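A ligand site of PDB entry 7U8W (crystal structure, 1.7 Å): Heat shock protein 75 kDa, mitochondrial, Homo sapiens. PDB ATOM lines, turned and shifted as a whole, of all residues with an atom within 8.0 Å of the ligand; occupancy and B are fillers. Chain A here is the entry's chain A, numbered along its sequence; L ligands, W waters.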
ATOM      1  N   TYR A 429       4.151  17.459  25.490  1.00  0.00           N
ATOM      2  CA  TYR A 429       3.780  16.065  25.327  1.00  0.00           C
ATOM      3  C   TYR A 429       2.434  15.959  24.629  1.00  0.00           C
ATOM      4  O   TYR A 429       1.519  16.748  24.884  1.00  0.00           O
ATOM      5  CB  TYR A 429       3.708  15.353  26.681  1.00  0.00           C
ATOM      6  CG  TYR A 429       5.058  15.282  27.328  1.00  0.00           C
ATOM      7  CD1 TYR A 429       5.972  14.312  26.941  1.00  0.00           C
ATOM      8  CD2 TYR A 429       5.456  16.228  28.283  1.00  0.00           C
ATOM      9  CE1 TYR A 429       7.235  14.258  27.513  1.00  0.00           C
ATOM     10  CE2 TYR A 429       6.719  16.173  28.855  1.00  0.00           C
ATOM     11  CZ  TYR A 429       7.594  15.181  28.474  1.00  0.00           C
ATOM     12  OH  TYR A 429       8.857  15.130  29.032  1.00  0.00           O
ATOM     13  N   TYR A 444      -0.174   4.885  29.358  1.00  0.00           N
ATOM     14  CA  TYR A 444       0.901   5.860  29.478  1.00  0.00           C
ATOM     15  C   TYR A 444       0.368   7.185  29.997  1.00  0.00           C
ATOM     16  O   TYR A 444       0.927   7.765  30.935  1.00  0.00           O
ATOM     17  CB  TYR A 444       1.623   6.028  28.140  1.00  0.00           C
ATOM     18  CG  TYR A 444       2.310   4.765  27.656  1.00  0.00           C
ATOM     19  CD1 TYR A 444       3.625   4.482  28.023  1.00  0.00           C
ATOM     20  CD2 TYR A 444       1.643   3.851  26.854  1.00  0.00           C
ATOM     21  CE1 TYR A 444       4.250   3.330  27.597  1.00  0.00           C
ATOM     22  CE2 TYR A 444       2.265   2.686  26.411  1.00  0.00           C
ATOM     23  CZ  TYR A 444       3.571   2.434  26.785  1.00  0.00           C
ATOM     24  OH  TYR A 444       4.186   1.273  26.356  1.00  0.00           O
ATOM     25  N   TYR A 445      -0.740   7.672  29.433  1.00  0.00           N
ATOM     26  CA  TYR A 445      -1.324   8.896  29.967  1.00  0.00           C
ATOM     27  C   TYR A 445      -1.787   8.699  31.407  1.00  0.00           C
ATOM     28  O   TYR A 445      -1.581   9.573  32.256  1.00  0.00           O
ATOM     29  CB  TYR A 445      -2.484   9.388  29.109  1.00  0.00           C
ATOM     30  CG  TYR A 445      -3.162  10.506  29.850  1.00  0.00           C
ATOM     31  CD1 TYR A 445      -2.499  11.707  30.057  1.00  0.00           C
ATOM     32  CD2 TYR A 445      -4.424  10.339  30.429  1.00  0.00           C
ATOM     33  CE1 TYR A 445      -3.061  12.716  30.781  1.00  0.00           C
ATOM     34  CE2 TYR A 445      -4.998  11.352  31.147  1.00  0.00           C
ATOM     35  CZ  TYR A 445      -4.313  12.537  31.322  1.00  0.00           C
ATOM     36  OH  TYR A 445      -4.864  13.555  32.049  1.00  0.00           O
ATOM     37  N   ALA A 447      -0.561   6.933  33.765  1.00  0.00           N
ATOM     38  CA  ALA A 447       0.558   7.039  34.699  1.00  0.00           C
ATOM     39  C   ALA A 447       1.047   8.481  34.804  1.00  0.00           C
ATOM     40  O   ALA A 447       1.367   8.955  35.901  1.00  0.00           O
ATOM     41  CB  ALA A 447       1.699   6.116  34.276  1.00  0.00           C
ATOM     42  N   MET A 448       1.091   9.198  33.668  1.00  0.00           N
ATOM     43  CA  MET A 448       1.578  10.573  33.676  1.00  0.00           C
ATOM     44  C   MET A 448       0.679  11.484  34.480  1.00  0.00           C
ATOM     45  O   MET A 448       1.147  12.462  35.062  1.00  0.00           O
ATOM     46  CB  MET A 448       1.690  11.103  32.252  1.00  0.00           C
ATOM     47  CG  MET A 448       2.848  10.486  31.466  1.00  0.00           C
ATOM     48  SD  MET A 448       2.854  11.090  29.767  1.00  0.00           S
ATOM     49  CE  MET A 448       3.211  12.837  30.001  1.00  0.00           C
ATOM     50  N   ILE A 479       7.009  15.643  22.072  1.00  0.00           N
ATOM     51  CA  ILE A 479       7.257  14.242  22.409  1.00  0.00           C
ATOM     52  C   ILE A 479       5.929  13.515  22.446  1.00  0.00           C
ATOM     53  O   ILE A 479       5.037  13.886  23.222  1.00  0.00           O
ATOM     54  CB  ILE A 479       7.981  14.104  23.756  1.00  0.00           C
ATOM     55  CG1 ILE A 479       9.322  14.829  23.712  1.00  0.00           C
ATOM     56  CG2 ILE A 479       8.163  12.626  24.120  1.00  0.00           C
ATOM     57  CD1 ILE A 479      10.103  14.712  24.996  1.00  0.00           C
ATOM     58  N   SER A 480       5.799  12.459  21.639  1.00  0.00           N
ATOM     59  CA  SER A 480       4.648  11.571  21.724  1.00  0.00           C
ATOM     60  C   SER A 480       4.784  10.650  22.935  1.00  0.00           C
ATOM     61  O   SER A 480       5.832  10.011  23.128  1.00  0.00           O
ATOM     62  CB  SER A 480       4.513  10.739  20.438  1.00  0.00           C
ATOM     63  OG  SER A 480       3.471   9.783  20.545  1.00  0.00           O
ATOM     64  N   VAL A 481       3.738  10.577  23.766  1.00  0.00           N
ATOM     65  CA  VAL A 481       3.868   9.784  24.986  1.00  0.00           C
ATOM     66  C   VAL A 481       3.748   8.293  24.724  1.00  0.00           C
ATOM     67  O   VAL A 481       4.063   7.491  25.613  1.00  0.00           O
ATOM     68  CB  VAL A 481       2.831  10.205  26.054  1.00  0.00           C
ATOM     69  CG1 VAL A 481       2.911  11.687  26.318  1.00  0.00           C
ATOM     70  CG2 VAL A 481       1.428   9.798  25.644  1.00  0.00           C
ATOM     71  N   GLU A 482       3.327   7.894  23.527  1.00  0.00           N
ATOM     72  CA  GLU A 482       3.397   6.508  23.087  1.00  0.00           C
ATOM     73  C   GLU A 482       4.271   6.431  21.841  1.00  0.00           C
ATOM     74  O   GLU A 482       4.197   7.306  20.981  1.00  0.00           O
ATOM     75  CB  GLU A 482       2.023   5.919  22.781  1.00  0.00           C
ATOM     76  CG  GLU A 482       1.123   5.805  23.987  1.00  0.00           C
ATOM     77  CD  GLU A 482      -0.062   4.903  23.737  1.00  0.00           C
ATOM     78  OE1 GLU A 482       0.000   4.081  22.791  1.00  0.00           O
ATOM     79  OE2 GLU A 482      -1.060   4.997  24.474  1.00  0.00           O
ATOM     80  N   THR A 483       5.064   5.386  21.739  1.00  0.00           N
ATOM     81  CA  THR A 483       5.942   5.217  20.580  1.00  0.00           C
ATOM     82  C   THR A 483       5.336   4.291  19.533  1.00  0.00           C
ATOM     83  O   THR A 483       5.843   4.220  18.396  1.00  0.00           O
ATOM     84  CB  THR A 483       7.299   4.653  20.992  1.00  0.00           C
ATOM     85  OG1 THR A 483       7.079   3.412  21.673  1.00  0.00           O
ATOM     86  CG2 THR A 483       8.044   5.632  21.896  1.00  0.00           C
HETATM   87  C1  LIG L   1       8.337   2.586  24.933  1.00  0.00           C
HETATM   88  C2  LIG L   1       8.158   1.656  25.977  1.00  0.00           C
HETATM   89  C3  LIG L   1       8.915   0.520  26.070  1.00  0.00           C
HETATM   90  C4  LIG L   1       9.817   0.290  25.073  1.00  0.00           C
HETATM   91  C5  LIG L   1       9.982   1.181  24.026  1.00  0.00           C
HETATM   92  C6  LIG L   1       9.224   2.345  23.925  1.00  0.00           C
HETATM   93  O1  LIG L   1       7.242   1.880  27.008  1.00  0.00           O
HETATM   94  C7  LIG L   1       7.381   3.763  24.987  1.00  0.00           C
HETATM   95  O2  LIG L   1       6.542   3.874  24.157  1.00  0.00           O
HETATM   96  N1  LIG L   1       7.448   4.643  26.104  1.00  0.00           N
HETATM   97  C8  LIG L   1      11.018   0.810  22.976  1.00  0.00           C
HETATM   98  O3  LIG L   1      12.068   0.374  23.328  1.00  0.00           O
HETATM   99  N2  LIG L   1      10.678   0.934  21.584  1.00  0.00           N
HETATM  100  C9  LIG L   1      11.502   0.609  20.580  1.00  0.00           C
HETATM  101  C10 LIG L   1      10.814   0.853  19.357  1.00  0.00           C
HETATM  102  C11 LIG L   1       9.568   1.336  19.687  1.00  0.00           C
HETATM  103  C12 LIG L   1       9.513   1.369  21.106  1.00  0.00           C
HETATM  104  C13 LIG L   1      11.173   0.716  18.003  1.00  0.00           C
HETATM  105  C14 LIG L   1      10.269   1.056  16.990  1.00  0.00           C
HETATM  106  C15 LIG L   1       8.999   1.541  17.332  1.00  0.00           C
HETATM  107  C16 LIG L   1       8.640   1.682  18.673  1.00  0.00           C
HETATM  108  C17 LIG L   1       8.355   4.531  27.063  1.00  0.00           C
HETATM  109  C18 LIG L   1       8.114   5.544  28.011  1.00  0.00           C
HETATM  110  C19 LIG L   1       7.030   6.252  27.540  1.00  0.00           C
HETATM  111  C20 LIG L   1       6.617   5.662  26.319  1.00  0.00           C
HETATM  112  C21 LIG L   1       8.758   5.898  29.215  1.00  0.00           C
HETATM  113  C22 LIG L   1       8.284   6.971  29.941  1.00  0.00           C
HETATM  114  C23 LIG L   1       7.188   7.681  29.476  1.00  0.00           C
HETATM  115  C24 LIG L   1       6.539   7.347  28.291  1.00  0.00           C
HETATM  116  F1  LIG L   1      12.405   0.231  17.694  1.00  0.00           F
HETATM  117  F2  LIG L   1       6.744   8.741  30.200  1.00  0.00           F
HETATM  118  O   HOH W   1       4.049   2.359  23.141  1.00  0.00           O
HETATM  119  O   HOH W   2      14.066   0.222  24.987  1.00  0.00           O
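The backbone NH (N) of Thr 483 sits at hydrogen-bond distance from an oxygen (O2) of the ligand (3.2 Å).
The side-chain hydroxyl (OG1) of Thr 483 is in hydrogen-bond range of an oxygen (O2) of the ligand (2.6 Å).
OH of Tyr 444 sits at hydrogen-bond distance from O1 of the ligand, at 3.2 Å.
Val 481 touches the ligand (O to C20, 3.2 Å).
Hydrophobic or aromatic side chains within 4 Å of the ligand: Tyr 444.
Of the 10 residues printed, 3 come within 4 Å of the ligand.
Along chain A the residues within 4 Å of the ligand span positions 444 to 483.
Water W1 lies within hydrogen-bond range of O2 of the ligand (3.1 Å), OH of Tyr 444 (3.4 Å) and N of Thr 483 (3.5 Å).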
